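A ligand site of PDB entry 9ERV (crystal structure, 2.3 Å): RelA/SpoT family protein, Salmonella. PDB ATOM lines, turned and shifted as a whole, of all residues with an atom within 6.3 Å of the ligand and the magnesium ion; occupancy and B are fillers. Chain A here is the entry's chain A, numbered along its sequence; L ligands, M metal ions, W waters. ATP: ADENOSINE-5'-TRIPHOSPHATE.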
ATOM      1  N   ALA A  76      16.782 -27.903  -4.117  1.00  0.00           N
ATOM      2  CA  ALA A  76      17.226 -27.059  -5.200  1.00  0.00           C
ATOM      3  C   ALA A  76      16.025 -26.568  -5.995  1.00  0.00           C
ATOM      4  O   ALA A  76      14.984 -27.220  -6.002  1.00  0.00           O
ATOM      5  CB  ALA A  76      18.146 -27.844  -6.127  1.00  0.00           C
ATOM      6  N   ARG A  77      16.187 -25.461  -6.725  1.00  0.00           N
ATOM      7  CA  ARG A  77      15.114 -24.955  -7.569  1.00  0.00           C
ATOM      8  C   ARG A  77      15.656 -24.228  -8.776  1.00  0.00           C
ATOM      9  O   ARG A  77      16.817 -23.810  -8.759  1.00  0.00           O
ATOM     10  CB  ARG A  77      14.080 -24.125  -6.749  1.00  0.00           C
ATOM     11  CG  ARG A  77      14.220 -22.617  -6.820  1.00  0.00           C
ATOM     12  CD  ARG A  77      15.188 -22.081  -5.811  1.00  0.00           C
ATOM     13  NE  ARG A  77      15.817 -20.871  -6.321  1.00  0.00           N
ATOM     14  CZ  ARG A  77      16.671 -20.108  -5.643  1.00  0.00           C
ATOM     15  NH1 ARG A  77      16.994 -20.431  -4.389  1.00  0.00           N
ATOM     16  NH2 ARG A  77      17.184 -19.025  -6.191  1.00  0.00           N
ATOM     17  N   ARG A  78      14.834 -24.092  -9.823  1.00  0.00           N
ATOM     18  CA  ARG A  78      15.298 -23.405 -10.999  1.00  0.00           C
ATOM     19  C   ARG A  78      14.143 -22.947 -11.869  1.00  0.00           C
ATOM     20  O   ARG A  78      13.173 -23.668 -12.087  1.00  0.00           O
ATOM     21  CB  ARG A  78      16.382 -24.233 -11.748  1.00  0.00           C
ATOM     22  CG  ARG A  78      16.201 -24.500 -13.231  1.00  0.00           C
ATOM     23  CD  ARG A  78      15.312 -25.669 -13.334  1.00  0.00           C
ATOM     24  NE  ARG A  78      14.844 -26.016 -14.664  1.00  0.00           N
ATOM     25  CZ  ARG A  78      13.572 -26.249 -14.959  1.00  0.00           C
ATOM     26  NH1 ARG A  78      12.614 -25.931 -14.099  1.00  0.00           N
ATOM     27  NH2 ARG A  78      13.241 -26.746 -16.135  1.00  0.00           N
ATOM     28  N   LYS A  80      13.111 -22.145 -15.478  1.00  0.00           N
ATOM     29  CA  LYS A  80      13.546 -22.600 -16.784  1.00  0.00           C
ATOM     30  C   LYS A  80      13.922 -21.404 -17.622  1.00  0.00           C
ATOM     31  O   LYS A  80      13.147 -20.474 -17.673  1.00  0.00           O
ATOM     32  CB  LYS A  80      12.410 -23.399 -17.444  1.00  0.00           C
ATOM     33  CG  LYS A  80      12.889 -24.400 -18.481  1.00  0.00           C
ATOM     34  CD  LYS A  80      11.748 -25.000 -19.267  1.00  0.00           C
ATOM     35  CE  LYS A  80      12.192 -26.247 -19.983  1.00  0.00           C
ATOM     36  NZ  LYS A  80      12.625 -27.288 -19.018  1.00  0.00           N
ATOM     37  N   ARG A  81      15.112 -21.403 -18.228  1.00  0.00           N
ATOM     38  CA  ARG A  81      15.618 -20.296 -19.048  1.00  0.00           C
ATOM     39  C   ARG A  81      14.732 -19.975 -20.257  1.00  0.00           C
ATOM     40  O   ARG A  81      14.127 -20.868 -20.833  1.00  0.00           O
ATOM     41  CB  ARG A  81      17.041 -20.641 -19.536  1.00  0.00           C
ATOM     42  CG  ARG A  81      18.150 -20.180 -18.588  1.00  0.00           C
ATOM     43  CD  ARG A  81      19.345 -21.124 -18.482  1.00  0.00           C
ATOM     44  NE  ARG A  81      19.692 -21.790 -19.739  1.00  0.00           N
ATOM     45  CZ  ARG A  81      20.709 -21.439 -20.522  1.00  0.00           C
ATOM     46  NH1 ARG A  81      21.489 -20.409 -20.202  1.00  0.00           N
ATOM     47  NH2 ARG A  81      20.951 -22.115 -21.647  1.00  0.00           N
ATOM     48  N   THR A  84      15.816 -21.911 -23.439  1.00  0.00           N
ATOM     49  CA  THR A  84      15.423 -23.320 -23.353  1.00  0.00           C
ATOM     50  C   THR A  84      13.955 -23.461 -23.740  1.00  0.00           C
ATOM     51  O   THR A  84      13.635 -24.353 -24.516  1.00  0.00           O
ATOM     52  CB  THR A  84      15.642 -23.849 -21.917  1.00  0.00           C
ATOM     53  OG1 THR A  84      16.947 -23.500 -21.474  1.00  0.00           O
ATOM     54  CG2 THR A  84      15.402 -25.342 -21.799  1.00  0.00           C
ATOM     55  N   LYS A  88      12.543 -25.418 -27.037  1.00  0.00           N
ATOM     56  CA  LYS A  88      11.612 -26.519 -26.850  1.00  0.00           C
ATOM     57  C   LYS A  88      10.406 -26.351 -27.769  1.00  0.00           C
ATOM     58  O   LYS A  88       9.995 -27.308 -28.414  1.00  0.00           O
ATOM     59  CB  LYS A  88      11.177 -26.593 -25.375  1.00  0.00           C
ATOM     60  CG  LYS A  88      10.792 -27.986 -24.926  1.00  0.00           C
ATOM     61  CD  LYS A  88      10.596 -28.054 -23.414  1.00  0.00           C
ATOM     62  CE  LYS A  88      10.458 -29.474 -22.953  1.00  0.00           C
ATOM     63  NZ  LYS A  88      11.533 -30.331 -23.527  1.00  0.00           N
ATOM     64  N   ASP A 110       6.857 -27.806 -15.924  1.00  0.00           N
ATOM     65  CA  ASP A 110       8.102 -27.473 -15.268  1.00  0.00           C
ATOM     66  C   ASP A 110       8.736 -26.121 -15.610  1.00  0.00           C
ATOM     67  O   ASP A 110       9.954 -26.015 -15.424  1.00  0.00           O
ATOM     68  CB  ASP A 110       9.124 -28.610 -15.548  1.00  0.00           C
ATOM     69  CG  ASP A 110       9.586 -28.638 -16.999  1.00  0.00           C
ATOM     70  OD1 ASP A 110       8.787 -28.266 -17.889  1.00  0.00           O
ATOM     71  OD2 ASP A 110      10.771 -28.999 -17.233  1.00  0.00           O
ATOM     72  N   GLY A 112       8.767 -23.642 -13.667  1.00  0.00           N
ATOM     73  CA  GLY A 112       9.405 -23.608 -12.362  1.00  0.00           C
ATOM     74  C   GLY A 112       9.550 -25.050 -11.927  1.00  0.00           C
ATOM     75  O   GLY A 112       8.658 -25.864 -12.151  1.00  0.00           O
ATOM     76  N   GLY A 113      10.705 -25.397 -11.361  1.00  0.00           N
ATOM     77  CA  GLY A 113      10.972 -26.758 -10.894  1.00  0.00           C
ATOM     78  C   GLY A 113      11.767 -26.755  -9.598  1.00  0.00           C
ATOM     79  O   GLY A 113      12.723 -26.000  -9.454  1.00  0.00           O
ATOM     80  N   CYS A 114      11.349 -27.584  -8.647  1.00  0.00           N
ATOM     81  CA  CYS A 114      11.928 -27.845  -7.322  1.00  0.00           C
ATOM     82  C   CYS A 114      12.420 -29.264  -7.264  1.00  0.00           C
ATOM     83  O   CYS A 114      11.820 -30.120  -7.875  1.00  0.00           O
ATOM     84  CB  CYS A 114      10.880 -27.636  -6.232  1.00  0.00           C
ATOM     85  SG  CYS A 114      10.533 -25.922  -5.928  1.00  0.00           S
ATOM     86  N   ARG A 115      13.401 -29.538  -6.420  1.00  0.00           N
ATOM     87  CA  ARG A 115      13.963 -30.863  -6.293  1.00  0.00           C
ATOM     88  C   ARG A 115      14.387 -31.158  -4.868  1.00  0.00           C
ATOM     89  O   ARG A 115      15.063 -30.341  -4.267  1.00  0.00           O
ATOM     90  CB  ARG A 115      15.165 -30.990  -7.251  1.00  0.00           C
ATOM     91  CG  ARG A 115      15.876 -32.340  -7.218  1.00  0.00           C
ATOM     92  CD  ARG A 115      17.076 -32.293  -8.119  1.00  0.00           C
ATOM     93  NE  ARG A 115      16.654 -32.304  -9.508  1.00  0.00           N
ATOM     94  CZ  ARG A 115      17.411 -31.952 -10.542  1.00  0.00           C
ATOM     95  NH1 ARG A 115      18.643 -31.517 -10.346  1.00  0.00           N
ATOM     96  NH2 ARG A 115      16.939 -32.043 -11.777  1.00  0.00           N
ATOM     97  N   GLU A 179       6.902 -28.058 -11.005  1.00  0.00           N
ATOM     98  CA  GLU A 179       7.240 -29.477 -10.905  1.00  0.00           C
ATOM     99  C   GLU A 179       8.074 -29.753  -9.670  1.00  0.00           C
ATOM    100  O   GLU A 179       8.968 -28.989  -9.360  1.00  0.00           O
ATOM    101  CB  GLU A 179       8.008 -29.930 -12.158  1.00  0.00           C
ATOM    102  CG  GLU A 179       8.325 -31.430 -12.143  1.00  0.00           C
ATOM    103  CD  GLU A 179       9.253 -31.879 -13.259  1.00  0.00           C
ATOM    104  OE1 GLU A 179      10.482 -31.710 -13.102  1.00  0.00           O
ATOM    105  OE2 GLU A 179       8.751 -32.378 -14.295  1.00  0.00           O
ATOM    106  N   VAL A 180       7.773 -30.840  -8.942  1.00  0.00           N
ATOM    107  CA  VAL A 180       8.558 -31.228  -7.791  1.00  0.00           C
ATOM    108  C   VAL A 180       9.231 -32.582  -8.038  1.00  0.00           C
ATOM    109  O   VAL A 180       8.536 -33.574  -8.222  1.00  0.00           O
ATOM    110  CB  VAL A 180       7.734 -31.184  -6.475  1.00  0.00           C
ATOM    111  CG1 VAL A 180       8.480 -31.885  -5.341  1.00  0.00           C
ATOM    112  CG2 VAL A 180       7.383 -29.759  -6.104  1.00  0.00           C
ATOM    113  N   GLN A 181      10.565 -32.645  -8.068  1.00  0.00           N
ATOM    114  CA  GLN A 181      11.282 -33.897  -8.289  1.00  0.00           C
ATOM    115  C   GLN A 181      11.808 -34.465  -6.962  1.00  0.00           C
ATOM    116  O   GLN A 181      12.395 -33.734  -6.170  1.00  0.00           O
ATOM    117  CB  GLN A 181      12.473 -33.679  -9.245  1.00  0.00           C
ATOM    118  CG  GLN A 181      12.082 -33.438 -10.701  1.00  0.00           C
ATOM    119  CD  GLN A 181      13.270 -33.113 -11.598  1.00  0.00           C
ATOM    120  OE1 GLN A 181      14.411 -32.985 -11.145  1.00  0.00           O
ATOM    121  NE2 GLN A 181      13.026 -32.892 -12.885  1.00  0.00           N
ATOM    122  N   ARG A 183      14.223 -37.498  -5.373  1.00  0.00           N
ATOM    123  CA  ARG A 183      15.307 -38.404  -5.763  1.00  0.00           C
ATOM    124  C   ARG A 183      16.140 -38.813  -4.571  1.00  0.00           C
ATOM    125  O   ARG A 183      16.340 -38.002  -3.691  1.00  0.00           O
ATOM    126  CB  ARG A 183      16.311 -37.618  -6.614  1.00  0.00           C
ATOM    127  CG  ARG A 183      16.178 -37.835  -8.044  1.00  0.00           C
ATOM    128  CD  ARG A 183      16.050 -36.456  -8.621  1.00  0.00           C
ATOM    129  NE  ARG A 183      17.343 -35.964  -9.067  1.00  0.00           N
ATOM    130  CZ  ARG A 183      17.596 -35.538 -10.306  1.00  0.00           C
ATOM    131  NH1 ARG A 183      16.638 -35.560 -11.221  1.00  0.00           N
ATOM    132  NH2 ARG A 183      18.806 -35.105 -10.622  1.00  0.00           N
ATOM    133  N   GLU A 195      24.491 -35.791 -16.880  1.00  0.00           N
ATOM    134  CA  GLU A 195      24.602 -34.429 -17.382  1.00  0.00           C
ATOM    135  C   GLU A 195      26.049 -34.009 -17.678  1.00  0.00           C
ATOM    136  O   GLU A 195      26.298 -33.382 -18.703  1.00  0.00           O
ATOM    137  CB  GLU A 195      23.896 -33.414 -16.494  1.00  0.00           C
ATOM    138  CG  GLU A 195      23.692 -32.117 -17.258  1.00  0.00           C
ATOM    139  CD  GLU A 195      22.573 -31.247 -16.729  1.00  0.00           C
ATOM    140  OE1 GLU A 195      21.528 -31.820 -16.335  1.00  0.00           O
ATOM    141  OE2 GLU A 195      22.739 -30.012 -16.707  1.00  0.00           O
ATOM    142  N   LYS A 206      19.482 -36.066 -25.100  1.00  0.00           N
ATOM    143  CA  LYS A 206      18.110 -35.596 -24.979  1.00  0.00           C
ATOM    144  C   LYS A 206      17.610 -35.047 -26.312  1.00  0.00           C
ATOM    145  O   LYS A 206      16.472 -35.338 -26.705  1.00  0.00           O
ATOM    146  CB  LYS A 206      17.972 -34.532 -23.874  1.00  0.00           C
ATOM    147  CG  LYS A 206      17.726 -35.119 -22.487  1.00  0.00           C
ATOM    148  CD  LYS A 206      16.981 -34.133 -21.591  1.00  0.00           C
ATOM    149  CE  LYS A 206      17.782 -32.878 -21.299  1.00  0.00           C
ATOM    150  NZ  LYS A 206      17.221 -31.683 -21.967  1.00  0.00           N
ATOM    151  N   ALA A 350      24.542 -25.709 -11.582  1.00  0.00           N
ATOM    152  CA  ALA A 350      23.460 -26.686 -11.587  1.00  0.00           C
ATOM    153  C   ALA A 350      23.686 -27.776 -10.527  1.00  0.00           C
ATOM    154  O   ALA A 350      22.729 -28.232  -9.884  1.00  0.00           O
ATOM    155  CB  ALA A 350      23.357 -27.311 -12.957  1.00  0.00           C
ATOM    156  N   TYR A 351      24.956 -28.177 -10.334  1.00  0.00           N
ATOM    157  CA  TYR A 351      25.304 -29.224  -9.380  1.00  0.00           C
ATOM    158  C   TYR A 351      26.357 -28.798  -8.341  1.00  0.00           C
ATOM    159  O   TYR A 351      27.539 -29.084  -8.504  1.00  0.00           O
ATOM    160  CB  TYR A 351      25.798 -30.462 -10.126  1.00  0.00           C
ATOM    161  CG  TYR A 351      24.774 -30.983 -11.107  1.00  0.00           C
ATOM    162  CD1 TYR A 351      23.619 -31.618 -10.675  1.00  0.00           C
ATOM    163  CD2 TYR A 351      24.936 -30.775 -12.468  1.00  0.00           C
ATOM    164  CE1 TYR A 351      22.688 -32.105 -11.571  1.00  0.00           C
ATOM    165  CE2 TYR A 351      23.987 -31.225 -13.378  1.00  0.00           C
ATOM    166  CZ  TYR A 351      22.864 -31.881 -12.922  1.00  0.00           C
ATOM    167  OH  TYR A 351      21.940 -32.342 -13.812  1.00  0.00           O
HETATM  168  PG  ATP L   1      13.400 -31.013 -20.312  1.00  0.00           P
HETATM  169  O1G ATP L   1      11.924 -30.860 -19.841  1.00  0.00           O
HETATM  170  O2G ATP L   1      13.597 -32.309 -21.132  1.00  0.00           O
HETATM  171  O3G ATP L   1      13.878 -29.772 -21.167  1.00  0.00           O
HETATM  172  PB  ATP L   1      15.183 -30.201 -18.120  1.00  0.00           P
HETATM  173  O1B ATP L   1      14.136 -29.489 -17.355  1.00  0.00           O
HETATM  174  O2B ATP L   1      16.024 -31.026 -17.145  1.00  0.00           O
HETATM  175  O3B ATP L   1      14.471 -31.202 -19.138  1.00  0.00           O
HETATM  176  PA  ATP L   1      16.733 -27.727 -18.386  1.00  0.00           P
HETATM  177  O1A ATP L   1      15.639 -26.856 -17.924  1.00  0.00           O
HETATM  178  O2A ATP L   1      17.484 -27.070 -19.546  1.00  0.00           O
HETATM  179  O3A ATP L   1      16.139 -29.140 -18.840  1.00  0.00           O
HETATM  180  O5' ATP L   1      17.802 -28.054 -17.222  1.00  0.00           O
HETATM  181  C5' ATP L   1      18.529 -27.047 -16.491  1.00  0.00           C
HETATM  182  C4' ATP L   1      18.987 -27.647 -15.180  1.00  0.00           C
HETATM  183  O4' ATP L   1      17.900 -27.609 -14.219  1.00  0.00           O
HETATM  184  C3' ATP L   1      19.457 -29.098 -15.224  1.00  0.00           C
HETATM  185  O3' ATP L   1      20.625 -29.261 -14.423  1.00  0.00           O
HETATM  186  C2' ATP L   1      18.287 -29.877 -14.629  1.00  0.00           C
HETATM  187  O2' ATP L   1      18.649 -31.077 -13.980  1.00  0.00           O
HETATM  188  C1' ATP L   1      17.763 -28.869 -13.605  1.00  0.00           C
HETATM  189  N9  ATP L   1      16.369 -29.070 -13.249  1.00  0.00           N
HETATM  190  C8  ATP L   1      15.354 -29.519 -14.051  1.00  0.00           C
HETATM  191  N7  ATP L   1      14.229 -29.727 -13.426  1.00  0.00           N
HETATM  192  C5  ATP L   1      14.501 -29.371 -12.112  1.00  0.00           C
HETATM  193  C6  ATP L   1      13.710 -29.347 -10.953  1.00  0.00           C
HETATM  194  N6  ATP L   1      12.479 -29.865 -10.871  1.00  0.00           N
HETATM  195  N1  ATP L   1      14.277 -28.845  -9.831  1.00  0.00           N
HETATM  196  C2  ATP L   1      15.548 -28.453  -9.857  1.00  0.00           C
HETATM  197  N3  ATP L   1      16.417 -28.483 -10.881  1.00  0.00           N
HETATM  198  C4  ATP L   1      15.820 -28.956 -11.993  1.00  0.00           C
HETATM  199 MG    MG M   1      12.012 -30.811 -17.200  1.00  0.00          MG
HETATM  200  O   HOH W   1      19.293 -24.540 -19.167  1.00  0.00           O
HETATM  201  O   HOH W   2      18.182 -23.635 -16.080  1.00  0.00           O
HETATM  202  O   HOH W   3      18.871 -27.263 -10.088  1.00  0.00           O
HETATM  203  O   HOH W   4      12.262 -34.827 -19.328  1.00  0.00           O
HETATM  204  O   HOH W   5      20.740 -29.220 -11.604  1.00  0.00           O
HETATM  205  O   HOH W   6      18.373 -32.423 -17.573  1.00  0.00           O
HETATM  206  O   HOH W   7      16.510 -24.148 -18.132  1.00  0.00           O
HETATM  207  O   HOH W   8      20.046 -33.974 -12.970  1.00  0.00           O
HETATM  208  O   HOH W   9      10.467 -33.857 -17.223  1.00  0.00           O
HETATM  209  O   HOH W  10      16.439 -28.689 -22.458  1.00  0.00           O
HETATM  210  O   HOH W  11      15.781 -32.873 -14.931  1.00  0.00           O
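NH1 of Arg 78 is in hydrogen-bond range of O of Asp 110 (3.0 Å).
The side-chain carboxylate (OD2) of Asp 110 lies close to the side-chain amino group (NZ) of Lys 80 (3.1 Å).
NH2 of Arg 115 lies within hydrogen-bond range of OE1 of Gln 181 (2.8 Å).
The backbone carbonyl oxygen of Gly 113 is in hydrogen-bond range of the backbone NH of Arg 78 (2.9 Å).
O of Cys 114 lies within hydrogen-bond range of N of Gln 181 (2.8 Å).
N of Cys 114 lies within hydrogen-bond range of O of Glu 179 (2.9 Å).
OH of Tyr 351 lies within hydrogen-bond range of OE1 of Glu 195.
The side-chain amide oxygen (OE1) of Gln 181 sits at hydrogen-bond distance from the guanidinium group (NH1) of Arg 183 (3.4 Å).
Water W6 lies within hydrogen-bond range of O2B of the ligand (2.8 Å) and OE1 of Glu 195 (3.4 Å).
Water W5 lies within hydrogen-bond range of O of Ala 350, O3' of the ligand and NH1 of Arg 115.
Water W11 lies within hydrogen-bond range of O2B of the ligand (2.9 Å), NE2 of Gln 181 (3.4 Å) and NH2 of Arg 115 (3.5 Å).
Water W10 lies within hydrogen-bond range of an oxygen (O3G) of the ligand (3.1 Å) and the side-chain amino group of Lys 206 (3.1 Å).
Water W1 lies within hydrogen-bond range of NE of Arg 81 (2.8 Å), O2A of the ligand (3.1 Å) and OG1 of Thr 84 (3.5 Å).
Water W8 lies within hydrogen-bond range of the side-chain hydroxyl of Tyr 351 (2.6 Å), the guanidinium group of Arg 183 (2.9 Å) and an oxygen (O2') of the ligand (3.4 Å).
OD2 of Asp 110 binds the magnesium ion.
The magnesium ion is bound by O1B of the ligand (2.5 Å).
Slightly farther from the magnesium ion lies an oxygen (O1G) of the ligand (2.6 Å).
Within 4 Å of the magnesium ion: Asp 110.
The nearest printed residue that does not touch the magnesium ion is Lys 80 (4.01 Å).
The backbone carbonyl oxygen (O) of Gly 113 lies close to a nitrogen (N1) of the ligand, 3.3 Å away.
Thr 84 touches the ligand.
Glu 179 touches the ligand.
Ala 350 touches the ligand.
Hydrophobic or aromatic side chains that line the ligand: Ala 350 and Tyr 351.
Within 4 Å of the ligand: Arg 78, Lys 80, Thr 84, Lys 88, Asp 110, Gly 113, Cys 114, Arg 115, Glu 179, Gln 181, Glu 195, Lys 206, Ala 350 and Tyr 351.
NH2 of Arg 115 lies within hydrogen-bond range of O2' of the ligand.
The guanidinium group (NH2) of Arg 78 lies within salt-bridge range of an oxygen (O1A) of the ligand (3.0 Å).
N of Cys 114 sits close to N1 of the ligand, 3.4 Å away.
A nitrogen (N6) of the ligand sits at hydrogen-bond distance from the backbone carbonyl oxygen (O) of Cys 114 (3.1 Å).
O1A of the ligand lies within salt-bridge range of NZ of Lys 80, 3.2 Å away.
The side-chain carboxylate (OE2) of Glu 195 sits at hydrogen-bond distance from an oxygen (O3') of the ligand (3.2 Å).
An oxygen (O3G) of the ligand is in salt-bridge range of the side-chain amino group of Lys 88 (3.4 Å).
The side-chain hydroxyl (OH) of Tyr 351 lies within hydrogen-bond range of an oxygen (O3') of the ligand, at 3.4 Å.
The side-chain amide nitrogen (NE2) of Gln 181 is in hydrogen-bond range of a nitrogen (N7) of the ligand (3.4 Å).
O2G of the ligand is in salt-bridge range of NZ of Lys 206, at 3.8 Å.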
